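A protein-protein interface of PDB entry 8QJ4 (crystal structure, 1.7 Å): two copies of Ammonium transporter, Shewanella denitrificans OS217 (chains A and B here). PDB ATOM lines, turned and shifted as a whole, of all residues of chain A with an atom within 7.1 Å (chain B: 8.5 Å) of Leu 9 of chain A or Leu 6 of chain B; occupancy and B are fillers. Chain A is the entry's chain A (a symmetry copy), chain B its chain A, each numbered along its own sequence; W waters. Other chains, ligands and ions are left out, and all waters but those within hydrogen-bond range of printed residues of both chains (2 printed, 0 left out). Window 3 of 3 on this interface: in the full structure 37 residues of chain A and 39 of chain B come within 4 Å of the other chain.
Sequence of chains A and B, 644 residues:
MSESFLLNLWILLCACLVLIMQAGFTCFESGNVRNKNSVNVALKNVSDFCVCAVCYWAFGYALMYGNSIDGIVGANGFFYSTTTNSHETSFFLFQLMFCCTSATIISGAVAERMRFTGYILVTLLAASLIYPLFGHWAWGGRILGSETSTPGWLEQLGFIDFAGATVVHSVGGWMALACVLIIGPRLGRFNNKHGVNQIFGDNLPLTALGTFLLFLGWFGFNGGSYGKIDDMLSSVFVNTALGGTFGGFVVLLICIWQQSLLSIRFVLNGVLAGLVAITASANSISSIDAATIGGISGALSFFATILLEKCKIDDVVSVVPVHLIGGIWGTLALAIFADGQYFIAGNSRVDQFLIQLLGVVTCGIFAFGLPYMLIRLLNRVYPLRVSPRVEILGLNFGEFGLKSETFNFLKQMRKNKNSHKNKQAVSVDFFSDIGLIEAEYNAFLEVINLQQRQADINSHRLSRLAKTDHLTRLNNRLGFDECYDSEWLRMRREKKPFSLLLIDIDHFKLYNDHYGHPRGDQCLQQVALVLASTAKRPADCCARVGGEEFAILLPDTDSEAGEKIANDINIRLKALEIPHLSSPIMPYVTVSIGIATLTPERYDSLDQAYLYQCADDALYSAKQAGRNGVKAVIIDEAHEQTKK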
ATOM      1  N   SER A   4     -26.333 -10.206  18.777  1.00  0.00           N
ATOM      2  CA  SER A   4     -26.941 -11.331  19.436  1.00  0.00           C
ATOM      3  C   SER A   4     -25.976 -12.530  19.511  1.00  0.00           C
ATOM      4  O   SER A   4     -26.375 -13.572  20.046  1.00  0.00           O
ATOM      5  CB  SER A   4     -28.232 -11.673  18.720  1.00  0.00           C
ATOM      6  OG  SER A   4     -27.970 -12.171  17.417  1.00  0.00           O
ATOM      7  N   PHE A   5     -24.717 -12.360  19.040  1.00  0.00           N
ATOM      8  CA  PHE A   5     -23.841 -13.497  18.782  1.00  0.00           C
ATOM      9  C   PHE A   5     -23.442 -14.143  20.091  1.00  0.00           C
ATOM     10  O   PHE A   5     -23.651 -15.351  20.205  1.00  0.00           O
ATOM     11  CB  PHE A   5     -22.574 -13.170  17.981  1.00  0.00           C
ATOM     12  CG  PHE A   5     -22.809 -12.798  16.542  1.00  0.00           C
ATOM     13  CD1 PHE A   5     -24.073 -12.903  15.959  1.00  0.00           C
ATOM     14  CD2 PHE A   5     -21.756 -12.332  15.767  1.00  0.00           C
ATOM     15  CE1 PHE A   5     -24.280 -12.518  14.643  1.00  0.00           C
ATOM     16  CE2 PHE A   5     -21.966 -11.958  14.441  1.00  0.00           C
ATOM     17  CZ  PHE A   5     -23.225 -12.058  13.884  1.00  0.00           C
ATOM     18  N   LEU A   6     -22.931 -13.358  21.057  1.00  0.00           N
ATOM     19  CA  LEU A   6     -22.411 -13.995  22.258  1.00  0.00           C
ATOM     20  C   LEU A   6     -23.514 -14.772  22.985  1.00  0.00           C
ATOM     21  O   LEU A   6     -23.278 -15.903  23.425  1.00  0.00           O
ATOM     22  CB  LEU A   6     -21.714 -12.982  23.166  1.00  0.00           C
ATOM     23  CG  LEU A   6     -21.121 -13.552  24.450  1.00  0.00           C
ATOM     24  CD1 LEU A   6     -20.121 -14.663  24.171  1.00  0.00           C
ATOM     25  CD2 LEU A   6     -20.463 -12.434  25.231  1.00  0.00           C
ATOM     26  N   LEU A   7     -24.726 -14.208  23.107  1.00  0.00           N
ATOM     27  CA  LEU A   7     -25.765 -14.926  23.821  1.00  0.00           C
ATOM     28  C   LEU A   7     -26.172 -16.211  23.084  1.00  0.00           C
ATOM     29  O   LEU A   7     -26.423 -17.231  23.738  1.00  0.00           O
ATOM     30  CB  LEU A   7     -26.980 -14.028  24.068  1.00  0.00           C
ATOM     31  CG  LEU A   7     -28.118 -14.642  24.884  1.00  0.00           C
ATOM     32  CD1 LEU A   7     -27.662 -15.142  26.236  1.00  0.00           C
ATOM     33  CD2 LEU A   7     -29.266 -13.623  25.104  1.00  0.00           C
ATOM     34  N   ASN A   8     -26.270 -16.156  21.745  1.00  0.00           N
ATOM     35  CA  ASN A   8     -26.603 -17.357  20.994  1.00  0.00           C
ATOM     36  C   ASN A   8     -25.545 -18.432  21.241  1.00  0.00           C
ATOM     37  O   ASN A   8     -25.872 -19.599  21.415  1.00  0.00           O
ATOM     38  CB  ASN A   8     -26.750 -17.122  19.489  1.00  0.00           C
ATOM     39  CG  ASN A   8     -28.164 -16.748  19.100  1.00  0.00           C
ATOM     40  OD1 ASN A   8     -29.138 -17.503  19.268  1.00  0.00           O
ATOM     41  ND2 ASN A   8     -28.294 -15.514  18.622  1.00  0.00           N
ATOM     42  N   LEU A   9     -24.267 -18.075  21.138  1.00  0.00           N
ATOM     43  CA  LEU A   9     -23.226 -19.064  21.305  1.00  0.00           C
ATOM     44  C   LEU A   9     -23.332 -19.652  22.711  1.00  0.00           C
ATOM     45  O   LEU A   9     -23.101 -20.838  22.846  1.00  0.00           O
ATOM     46  CB  LEU A   9     -21.858 -18.429  21.111  1.00  0.00           C
ATOM     47  CG  LEU A   9     -21.575 -17.877  19.713  1.00  0.00           C
ATOM     48  CD1 LEU A   9     -20.097 -17.559  19.551  1.00  0.00           C
ATOM     49  CD2 LEU A   9     -21.980 -18.829  18.648  1.00  0.00           C
ATOM     50  N   TRP A  10     -23.546 -18.800  23.728  1.00  0.00           N
ATOM     51  CA  TRP A  10     -23.708 -19.242  25.096  1.00  0.00           C
ATOM     52  C   TRP A  10     -24.842 -20.276  25.237  1.00  0.00           C
ATOM     53  O   TRP A  10     -24.622 -21.340  25.848  1.00  0.00           O
ATOM     54  CB  TRP A  10     -23.938 -18.043  26.031  1.00  0.00           C
ATOM     55  CG  TRP A  10     -24.138 -18.405  27.457  1.00  0.00           C
ATOM     56  CD1 TRP A  10     -25.281 -18.336  28.170  1.00  0.00           C
ATOM     57  CD2 TRP A  10     -23.144 -18.918  28.370  1.00  0.00           C
ATOM     58  NE1 TRP A  10     -25.079 -18.754  29.452  1.00  0.00           N
ATOM     59  CE2 TRP A  10     -23.769 -19.110  29.605  1.00  0.00           C
ATOM     60  CE3 TRP A  10     -21.787 -19.209  28.246  1.00  0.00           C
ATOM     61  CZ2 TRP A  10     -23.079 -19.610  30.721  1.00  0.00           C
ATOM     62  CZ3 TRP A  10     -21.094 -19.655  29.356  1.00  0.00           C
ATOM     63  CH2 TRP A  10     -21.734 -19.855  30.562  1.00  0.00           C
ATOM     64  N   ILE A  11     -26.027 -19.981  24.691  1.00  0.00           N
ATOM     65  CA  ILE A  11     -27.164 -20.867  24.800  1.00  0.00           C
ATOM     66  C   ILE A  11     -26.849 -22.202  24.092  1.00  0.00           C
ATOM     67  O   ILE A  11     -27.239 -23.269  24.602  1.00  0.00           O
ATOM     68  CB  ILE A  11     -28.457 -20.236  24.265  1.00  0.00           C
ATOM     69  CG1 ILE A  11     -28.841 -18.956  25.015  1.00  0.00           C
ATOM     70  CG2 ILE A  11     -29.627 -21.214  24.250  1.00  0.00           C
ATOM     71  CD1 ILE A  11     -29.038 -19.123  26.454  1.00  0.00           C
ATOM     72  N   LEU A  12     -26.197 -22.133  22.918  1.00  0.00           N
ATOM     73  CA  LEU A  12     -25.854 -23.363  22.218  1.00  0.00           C
ATOM     74  C   LEU A  12     -24.877 -24.249  23.015  1.00  0.00           C
ATOM     75  O   LEU A  12     -25.062 -25.466  23.065  1.00  0.00           O
ATOM     76  CB  LEU A  12     -25.252 -23.027  20.859  1.00  0.00           C
ATOM     77  CG  LEU A  12     -26.193 -22.385  19.832  1.00  0.00           C
ATOM     78  CD1 LEU A  12     -25.430 -22.026  18.596  1.00  0.00           C
ATOM     79  CD2 LEU A  12     -27.344 -23.274  19.480  1.00  0.00           C
ATOM     80  N   LEU A  13     -23.860 -23.653  23.652  1.00  0.00           N
ATOM     81  CA  LEU A  13     -22.960 -24.433  24.500  1.00  0.00           C
ATOM     82  C   LEU A  13     -23.682 -24.976  25.724  1.00  0.00           C
ATOM     83  O   LEU A  13     -23.433 -26.124  26.092  1.00  0.00           O
ATOM     84  CB  LEU A  13     -21.767 -23.564  24.859  1.00  0.00           C
ATOM     85  CG  LEU A  13     -20.861 -23.236  23.694  1.00  0.00           C
ATOM     86  CD1 LEU A  13     -19.911 -22.082  24.003  1.00  0.00           C
ATOM     87  CD2 LEU A  13     -20.075 -24.426  23.274  1.00  0.00           C
ATOM     88  N   CYS A  14     -24.589 -24.217  26.312  1.00  0.00           N
ATOM     89  CA  CYS A  14     -25.382 -24.671  27.440  1.00  0.00           C
ATOM     90  C   CYS A  14     -26.290 -25.842  27.024  1.00  0.00           C
ATOM     91  O   CYS A  14     -26.439 -26.783  27.824  1.00  0.00           O
ATOM     92  CB  CYS A  14     -26.174 -23.550  28.106  1.00  0.00           C
ATOM     93  SG  CYS A  14     -25.086 -22.390  28.995  1.00  0.00           S
ATOM     94  N   ALA A  15     -26.847 -25.815  25.806  1.00  0.00           N
ATOM     95  CA  ALA A  15     -27.676 -26.908  25.322  1.00  0.00           C
ATOM     96  C   ALA A  15     -26.807 -28.174  25.158  1.00  0.00           C
ATOM     97  O   ALA A  15     -27.318 -29.283  25.406  1.00  0.00           O
ATOM     98  CB  ALA A  15     -28.307 -26.539  23.998  1.00  0.00           C
ATOM     99  N   SER A  90     -31.762 -20.951  19.037  1.00  0.00           N
ATOM    100  CA  SER A  90     -30.934 -21.392  20.156  1.00  0.00           C
ATOM    101  C   SER A  90     -31.808 -21.792  21.354  1.00  0.00           C
ATOM    102  O   SER A  90     -31.619 -22.846  21.972  1.00  0.00           O
ATOM    103  CB  SER A  90     -29.954 -20.287  20.533  1.00  0.00           C
ATOM    104  OG  SER A  90     -28.940 -20.121  19.556  1.00  0.00           O
ATOM    105  N   GLU B   3     -12.794  -8.038  16.807  1.00  0.00           N
ATOM    106  CA  GLU B   3     -11.596  -8.850  17.142  1.00  0.00           C
ATOM    107  C   GLU B   3     -11.869 -10.320  16.837  1.00  0.00           C
ATOM    108  O   GLU B   3     -12.987 -10.832  16.947  1.00  0.00           O
ATOM    109  CB  GLU B   3     -11.121  -8.640  18.585  1.00  0.00           C
ATOM    110  CG  GLU B   3      -9.961  -7.654  18.659  1.00  0.00           C
ATOM    111  CD  GLU B   3      -9.549  -7.151  20.030  1.00  0.00           C
ATOM    112  OE1 GLU B   3     -10.211  -7.506  21.020  1.00  0.00           O
ATOM    113  OE2 GLU B   3      -8.566  -6.385  20.096  1.00  0.00           O
ATOM    114  N   SER B   4     -10.776 -10.991  16.465  1.00  0.00           N
ATOM    115  CA  SER B   4     -10.807 -12.384  16.105  1.00  0.00           C
ATOM    116  C   SER B   4     -11.116 -13.274  17.325  1.00  0.00           C
ATOM    117  O   SER B   4     -11.162 -14.499  17.160  1.00  0.00           O
ATOM    118  CB  SER B   4      -9.490 -12.743  15.447  1.00  0.00           C
ATOM    119  OG  SER B   4      -8.423 -12.678  16.381  1.00  0.00           O
ATOM    120  N   PHE B   5     -11.381 -12.662  18.504  1.00  0.00           N
ATOM    121  CA  PHE B   5     -11.377 -13.400  19.762  1.00  0.00           C
ATOM    122  C   PHE B   5     -12.553 -14.353  19.800  1.00  0.00           C
ATOM    123  O   PHE B   5     -12.307 -15.538  20.026  1.00  0.00           O
ATOM    124  CB  PHE B   5     -11.398 -12.530  21.024  1.00  0.00           C
ATOM    125  CG  PHE B   5     -10.141 -11.744  21.278  1.00  0.00           C
ATOM    126  CD1 PHE B   5      -8.997 -11.928  20.499  1.00  0.00           C
ATOM    127  CD2 PHE B   5     -10.105 -10.805  22.299  1.00  0.00           C
ATOM    128  CE1 PHE B   5      -7.859 -11.166  20.721  1.00  0.00           C
ATOM    129  CE2 PHE B   5      -8.956 -10.051  22.526  1.00  0.00           C
ATOM    130  CZ  PHE B   5      -7.836 -10.239  21.740  1.00  0.00           C
ATOM    131  N   LEU B   6     -13.778 -13.860  19.541  1.00  0.00           N
ATOM    132  CA  LEU B   6     -14.924 -14.737  19.722  1.00  0.00           C
ATOM    133  C   LEU B   6     -14.834 -15.952  18.792  1.00  0.00           C
ATOM    134  O   LEU B   6     -15.100 -17.078  19.229  1.00  0.00           O
ATOM    135  CB  LEU B   6     -16.239 -13.973  19.558  1.00  0.00           C
ATOM    136  CG  LEU B   6     -17.505 -14.802  19.740  1.00  0.00           C
ATOM    137  CD1 LEU B   6     -17.552 -15.481  21.100  1.00  0.00           C
ATOM    138  CD2 LEU B   6     -18.714 -13.908  19.556  1.00  0.00           C
ATOM    139  N   LEU B   7     -14.442 -15.764  17.523  1.00  0.00           N
ATOM    140  CA  LEU B   7     -14.384 -16.907  16.631  1.00  0.00           C
ATOM    141  C   LEU B   7     -13.305 -17.910  17.068  1.00  0.00           C
ATOM    142  O   LEU B   7     -13.530 -19.123  16.969  1.00  0.00           O
ATOM    143  CB  LEU B   7     -14.162 -16.460  15.183  1.00  0.00           C
ATOM    144  CG  LEU B   7     -14.160 -17.567  14.128  1.00  0.00           C
ATOM    145  CD1 LEU B   7     -15.429 -18.388  14.142  1.00  0.00           C
ATOM    146  CD2 LEU B   7     -13.973 -16.986  12.703  1.00  0.00           C
ATOM    147  N   ASN B   8     -12.137 -17.415  17.511  1.00  0.00           N
ATOM    148  CA  ASN B   8     -11.101 -18.319  17.985  1.00  0.00           C
ATOM    149  C   ASN B   8     -11.626 -19.136  19.165  1.00  0.00           C
ATOM    150  O   ASN B   8     -11.379 -20.332  19.254  1.00  0.00           O
ATOM    151  CB  ASN B   8      -9.805 -17.613  18.389  1.00  0.00           C
ATOM    152  CG  ASN B   8      -8.844 -17.466  17.229  1.00  0.00           C
ATOM    153  OD1 ASN B   8      -8.349 -18.436  16.627  1.00  0.00           O
ATOM    154  ND2 ASN B   8      -8.618 -16.209  16.858  1.00  0.00           N
ATOM    155  N   LEU B   9     -12.248 -18.479  20.142  1.00  0.00           N
ATOM    156  CA  LEU B   9     -12.714 -19.193  21.309  1.00  0.00           C
ATOM    157  C   LEU B   9     -13.731 -20.244  20.864  1.00  0.00           C
ATOM    158  O   LEU B   9     -13.727 -21.313  21.441  1.00  0.00           O
ATOM    159  CB  LEU B   9     -13.360 -18.232  22.293  1.00  0.00           C
ATOM    160  CG  LEU B   9     -12.430 -17.176  22.896  1.00  0.00           C
ATOM    161  CD1 LEU B   9     -13.095 -16.488  24.077  1.00  0.00           C
ATOM    162  CD2 LEU B   9     -11.143 -17.762  23.344  1.00  0.00           C
ATOM    163  N   TRP B  10     -14.650 -19.876  19.956  1.00  0.00           N
ATOM    164  CA  TRP B  10     -15.636 -20.793  19.426  1.00  0.00           C
ATOM    165  C   TRP B  10     -14.984 -22.043  18.805  1.00  0.00           C
ATOM    166  O   TRP B  10     -15.400 -23.172  19.135  1.00  0.00           O
ATOM    167  CB  TRP B  10     -16.546 -20.085  18.408  1.00  0.00           C
ATOM    168  CG  TRP B  10     -17.577 -20.959  17.793  1.00  0.00           C
ATOM    169  CD1 TRP B  10     -17.621 -21.410  16.524  1.00  0.00           C
ATOM    170  CD2 TRP B  10     -18.743 -21.513  18.442  1.00  0.00           C
ATOM    171  NE1 TRP B  10     -18.721 -22.192  16.325  1.00  0.00           N
ATOM    172  CE2 TRP B  10     -19.434 -22.265  17.488  1.00  0.00           C
ATOM    173  CE3 TRP B  10     -19.259 -21.419  19.733  1.00  0.00           C
ATOM    174  CZ2 TRP B  10     -20.621 -22.948  17.793  1.00  0.00           C
ATOM    175  CZ3 TRP B  10     -20.453 -22.051  20.024  1.00  0.00           C
ATOM    176  CH2 TRP B  10     -21.111 -22.803  19.071  1.00  0.00           C
ATOM    177  N   ILE B  11     -13.989 -21.860  17.929  1.00  0.00           N
ATOM    178  CA  ILE B  11     -13.338 -22.966  17.265  1.00  0.00           C
ATOM    179  C   ILE B  11     -12.635 -23.857  18.311  1.00  0.00           C
ATOM    180  O   ILE B  11     -12.660 -25.094  18.174  1.00  0.00           O
ATOM    181  CB  ILE B  11     -12.366 -22.506  16.171  1.00  0.00           C
ATOM    182  CG1 ILE B  11     -13.058 -21.697  15.070  1.00  0.00           C
ATOM    183  CG2 ILE B  11     -11.576 -23.661  15.563  1.00  0.00           C
ATOM    184  CD1 ILE B  11     -14.141 -22.396  14.380  1.00  0.00           C
ATOM    185  N   LEU B  12     -11.984 -23.233  19.310  1.00  0.00           N
ATOM    186  CA  LEU B  12     -11.323 -24.025  20.337  1.00  0.00           C
ATOM    187  C   LEU B  12     -12.310 -24.881  21.155  1.00  0.00           C
ATOM    188  O   LEU B  12     -12.019 -26.046  21.431  1.00  0.00           O
ATOM    189  CB  LEU B  12     -10.545 -23.104  21.269  1.00  0.00           C
ATOM    190  CG  LEU B  12      -9.335 -22.381  20.663  1.00  0.00           C
ATOM    191  CD1 LEU B  12      -8.744 -21.446  21.671  1.00  0.00           C
ATOM    192  CD2 LEU B  12      -8.287 -23.332  20.177  1.00  0.00           C
ATOM    193  N   LEU B  13     -13.472 -24.326  21.523  1.00  0.00           N
ATOM    194  CA  LEU B  13     -14.483 -25.122  22.217  1.00  0.00           C
ATOM    195  C   LEU B  13     -15.048 -26.211  21.317  1.00  0.00           C
ATOM    196  O   LEU B  13     -15.255 -27.323  21.799  1.00  0.00           O
ATOM    197  CB  LEU B  13     -15.553 -24.182  22.744  1.00  0.00           C
ATOM    198  CG  LEU B  13     -15.088 -23.266  23.854  1.00  0.00           C
ATOM    199  CD1 LEU B  13     -16.051 -22.107  24.093  1.00  0.00           C
ATOM    200  CD2 LEU B  13     -14.892 -24.018  25.122  1.00  0.00           C
ATOM    201  N   CYS B  14     -15.240 -25.937  20.039  1.00  0.00           N
ATOM    202  CA  CYS B  14     -15.705 -26.929  19.084  1.00  0.00           C
ATOM    203  C   CYS B  14     -14.670 -28.057  18.931  1.00  0.00           C
ATOM    204  O   CYS B  14     -15.085 -29.225  18.828  1.00  0.00           O
ATOM    205  CB  CYS B  14     -16.093 -26.328  17.737  1.00  0.00           C
ATOM    206  SG  CYS B  14     -17.615 -25.334  17.853  1.00  0.00           S
ATOM    207  N   HIS B  87      -6.537 -16.675  12.887  1.00  0.00           N
ATOM    208  CA  HIS B  87      -7.471 -17.780  13.063  1.00  0.00           C
ATOM    209  C   HIS B  87      -6.847 -19.134  12.758  1.00  0.00           C
ATOM    210  O   HIS B  87      -7.483 -20.169  13.024  1.00  0.00           O
ATOM    211  CB  HIS B  87      -8.725 -17.596  12.227  1.00  0.00           C
ATOM    212  CG  HIS B  87      -9.501 -16.410  12.631  1.00  0.00           C
ATOM    213  ND1 HIS B  87      -9.285 -15.201  11.994  1.00  0.00           N
ATOM    214  CD2 HIS B  87     -10.386 -16.161  13.603  1.00  0.00           C
ATOM    215  CE1 HIS B  87     -10.057 -14.264  12.555  1.00  0.00           C
ATOM    216  NE2 HIS B  87     -10.715 -14.809  13.552  1.00  0.00           N
ATOM    217  N   SER B  90      -6.164 -22.095  15.810  1.00  0.00           N
ATOM    218  CA  SER B  90      -7.434 -22.693  16.208  1.00  0.00           C
ATOM    219  C   SER B  90      -7.928 -23.678  15.139  1.00  0.00           C
ATOM    220  O   SER B  90      -8.336 -24.807  15.434  1.00  0.00           O
ATOM    221  CB  SER B  90      -8.459 -21.595  16.463  1.00  0.00           C
ATOM    222  OG  SER B  90      -8.175 -20.867  17.645  1.00  0.00           O
ATOM    223  N   GLY B 223     -20.483 -27.313  14.258  1.00  0.00           N
ATOM    224  CA  GLY B 223     -20.345 -25.941  14.670  1.00  0.00           C
ATOM    225  C   GLY B 223     -19.004 -25.312  14.334  1.00  0.00           C
ATOM    226  O   GLY B 223     -18.948 -24.124  13.973  1.00  0.00           O
ATOM    227  N   TYR B 226     -18.388 -24.061  10.588  1.00  0.00           N
ATOM    228  CA  TYR B 226     -19.259 -23.030  10.041  1.00  0.00           C
ATOM    229  C   TYR B 226     -18.470 -21.849   9.468  1.00  0.00           C
ATOM    230  O   TYR B 226     -18.982 -21.146   8.595  1.00  0.00           O
ATOM    231  CB  TYR B 226     -20.187 -22.513  11.114  1.00  0.00           C
ATOM    232  CG  TYR B 226     -21.374 -21.690  10.639  1.00  0.00           C
ATOM    233  CD1 TYR B 226     -22.397 -22.269   9.916  1.00  0.00           C
ATOM    234  CD2 TYR B 226     -21.499 -20.337  10.961  1.00  0.00           C
ATOM    235  CE1 TYR B 226     -23.502 -21.544   9.490  1.00  0.00           C
ATOM    236  CE2 TYR B 226     -22.612 -19.599  10.560  1.00  0.00           C
ATOM    237  CZ  TYR B 226     -23.620 -20.209   9.837  1.00  0.00           C
ATOM    238  OH  TYR B 226     -24.746 -19.546   9.442  1.00  0.00           O
ATOM    239  N   LYS B 228     -17.335 -19.007  10.773  1.00  0.00           N
ATOM    240  CA  LYS B 228     -17.622 -17.605  11.017  1.00  0.00           C
ATOM    241  C   LYS B 228     -18.621 -17.636  12.133  1.00  0.00           C
ATOM    242  O   LYS B 228     -18.953 -18.760  12.568  1.00  0.00           O
ATOM    243  CB  LYS B 228     -18.396 -16.932   9.897  1.00  0.00           C
ATOM    244  CG  LYS B 228     -19.745 -17.570   9.580  1.00  0.00           C
ATOM    245  CD  LYS B 228     -19.880 -17.759   8.052  1.00  0.00           C
ATOM    246  CE  LYS B 228     -20.976 -18.673   7.563  1.00  0.00           C
ATOM    247  NZ  LYS B 228     -22.138 -17.916   7.040  1.00  0.00           N
ATOM    248  N   ILE B 229     -19.159 -16.457  12.440  1.00  0.00           N
ATOM    249  CA  ILE B 229     -20.355 -16.449  13.247  1.00  0.00           C
ATOM    250  C   ILE B 229     -21.351 -15.506  12.583  1.00  0.00           C
ATOM    251  O   ILE B 229     -20.991 -14.391  12.223  1.00  0.00           O
ATOM    252  CB  ILE B 229     -20.047 -16.059  14.692  1.00  0.00           C
ATOM    253  CG1 ILE B 229     -19.106 -17.067  15.371  1.00  0.00           C
ATOM    254  CG2 ILE B 229     -21.360 -15.896  15.454  1.00  0.00           C
ATOM    255  CD1 ILE B 229     -18.175 -16.398  16.332  1.00  0.00           C
ATOM    256  N   ASP B 230     -22.569 -15.999  12.376  1.00  0.00           N
ATOM    257  CA  ASP B 230     -23.699 -15.170  11.987  1.00  0.00           C
ATOM    258  C   ASP B 230     -24.945 -15.719  12.691  1.00  0.00           C
ATOM    259  O   ASP B 230     -24.886 -16.652  13.518  1.00  0.00           O
ATOM    260  CB  ASP B 230     -23.765 -15.055  10.458  1.00  0.00           C
ATOM    261  CG  ASP B 230     -24.188 -16.320   9.754  1.00  0.00           C
ATOM    262  OD1 ASP B 230     -24.888 -17.179  10.408  1.00  0.00           O
ATOM    263  OD2 ASP B 230     -23.863 -16.448   8.560  1.00  0.00           O
ATOM    264  N   ASP B 231     -26.101 -15.136  12.344  1.00  0.00           N
ATOM    265  CA  ASP B 231     -27.331 -15.430  13.063  1.00  0.00           C
ATOM    266  C   ASP B 231     -27.942 -16.762  12.613  1.00  0.00           C
ATOM    267  O   ASP B 231     -28.982 -17.135  13.153  1.00  0.00           O
ATOM    268  CB  ASP B 231     -28.368 -14.304  12.898  1.00  0.00           C
ATOM    269  CG  ASP B 231     -28.963 -14.115  11.501  1.00  0.00           C
ATOM    270  OD1 ASP B 231     -28.428 -14.689  10.513  1.00  0.00           O
ATOM    271  OD2 ASP B 231     -29.975 -13.359  11.399  1.00  0.00           O
ATOM    272  N   LEU B 233     -26.113 -19.643  12.683  1.00  0.00           N
ATOM    273  CA  LEU B 233     -25.317 -20.735  13.281  1.00  0.00           C
ATOM    274  C   LEU B 233     -26.203 -21.662  14.099  1.00  0.00           C
ATOM    275  O   LEU B 233     -26.026 -22.882  14.065  1.00  0.00           O
ATOM    276  CB  LEU B 233     -24.219 -20.110  14.124  1.00  0.00           C
ATOM    277  CG  LEU B 233     -23.294 -21.068  14.880  1.00  0.00           C
ATOM    278  CD1 LEU B 233     -22.698 -22.138  13.987  1.00  0.00           C
ATOM    279  CD2 LEU B 233     -22.168 -20.297  15.536  1.00  0.00           C
ATOM    280  N   SER B 234     -27.178 -21.111  14.852  1.00  0.00           N
ATOM    281  CA  SER B 234     -28.017 -21.947  15.697  1.00  0.00           C
ATOM    282  C   SER B 234     -28.816 -22.960  14.860  1.00  0.00           C
ATOM    283  O   SER B 234     -29.174 -24.051  15.331  1.00  0.00           O
ATOM    284  CB  SER B 234     -28.849 -21.133  16.662  1.00  0.00           C
ATOM    285  OG  SER B 234     -29.709 -20.288  15.924  1.00  0.00           O
ATOM    286  N   PHE B 237     -27.107 -26.286  14.572  1.00  0.00           N
ATOM    287  CA  PHE B 237     -27.253 -27.069  15.804  1.00  0.00           C
ATOM    288  C   PHE B 237     -28.623 -27.744  15.868  1.00  0.00           C
ATOM    289  O   PHE B 237     -28.709 -28.939  16.104  1.00  0.00           O
ATOM    290  CB  PHE B 237     -27.037 -26.197  17.038  1.00  0.00           C
ATOM    291  CG  PHE B 237     -25.587 -25.981  17.393  1.00  0.00           C
ATOM    292  CD1 PHE B 237     -24.726 -25.348  16.529  1.00  0.00           C
ATOM    293  CD2 PHE B 237     -25.073 -26.462  18.602  1.00  0.00           C
ATOM    294  CE1 PHE B 237     -23.381 -25.169  16.859  1.00  0.00           C
ATOM    295  CE2 PHE B 237     -23.737 -26.283  18.907  1.00  0.00           C
ATOM    296  CZ  PHE B 237     -22.888 -25.697  18.030  1.00  0.00           C
HETATM  297  O   HOH W   1     -29.096 -16.354  15.428  1.00  0.00           O
HETATM  298  O   HOH W   2     -30.849 -18.437  17.663  1.00  0.00           O
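OD1 of Asn 8 of chain A lies within hydrogen-bond range of OG of Ser 90 of chain A (2.6 Å). The side-chain hydroxyl of Tyr 226 of chain B is in hydrogen-bond range of the side-chain carboxylate of Asp 230 of chain B (2.6 Å). The side-chain amino group (NZ) of Lys 228 of chain B lies within salt-bridge range of the side-chain carboxylate (OD2) of Asp 230 of chain B, 2.7 Å away.
Of chain B, only Leu 6, Trp 10, Ile 229 and Leu 233 come within 4 Å of Leu 9 of chain A. Printed residues of chain A within 4 Å of Leu 6 of chain B: Leu 9 (3.6 Å). Of the printed residues of chain A, Asp 230 of chain B touches Phe 5. Printed residues of chain B within 4 Å of Ser 90 of chain A: Ser 234. Of the printed residues of chain A, Ile 229 of chain B touches Phe 5 (3.4 Å) and Leu 9 (3.9 Å). Of the printed residues of chain A, Leu 13 of chain B touches Leu 13. Lys 228 of chain B touches none of the printed residues of chain A. The nearest printed residue of chain A that does not touch Ile 229 of chain B is Leu 6 of chain A (6.3 Å).
Among the printed residues, pairs that only touch across the chains: Phe 5 of chain A with Ile 229 of chain B, Phe 5 of chain A with Asp 230 of chain B, Phe 5 of chain A with Asp 231 of chain B, Leu 9 of chain A with Leu 6 of chain B, Leu 9 of chain A with Trp 10 of chain B, Leu 9 of chain A with Ile 229 of chain B, Leu 9 of chain A with Leu 233 of chain B, Leu 12 of chain A with Ser 234 of chain B, Leu 12 of chain A with Phe 237 of chain B, Leu 13 of chain A with Trp 10 of chain B, Leu 13 of chain A with Leu 13 of chain B and Ser 90 of chain A with Ser 234 of chain B.
Water W1 bridges O of Asp 231 of chain B and ND2 of Asn 8 of chain A. Water W2 lies within hydrogen-bond range of the side-chain amide oxygen of Asn 8 of chain A (2.5 Å), the side-chain hydroxyl of Ser 234 of chain B (2.8 Å) and the backbone NH of Ser 90 of chain A (3.0 Å).
Leu 9 of chain A touches Leu 6 of chain B, but with the chains exchanged Leu 6 of chain A does not touch Leu 9 of chain B (7.3 Å). Leu 13 of chain A touches Trp 10 of chain B, but with the chains exchanged Trp 10 of chain A does not touch Leu 13 of chain B (7.7 Å). Leu 13 of chain B touches its own counterpart, Leu 13 of chain A. 12 positions are printed for both chains.
Printed residues of chain A that touch a printed residue of chain B: Phe 5, Leu 9, Leu 12, Leu 13 and Ser 90. Hydrophobic or aromatic side chains of chain A within 4 Å of the printed part of chain B: Phe 5, Leu 9, Leu 12 and Leu 13. Hydrophobic or aromatic side chains of chain B within 4 Å of the printed part of chain A: Leu 6, Trp 10, Leu 13, Ile 229, Leu 233 and Phe 237.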
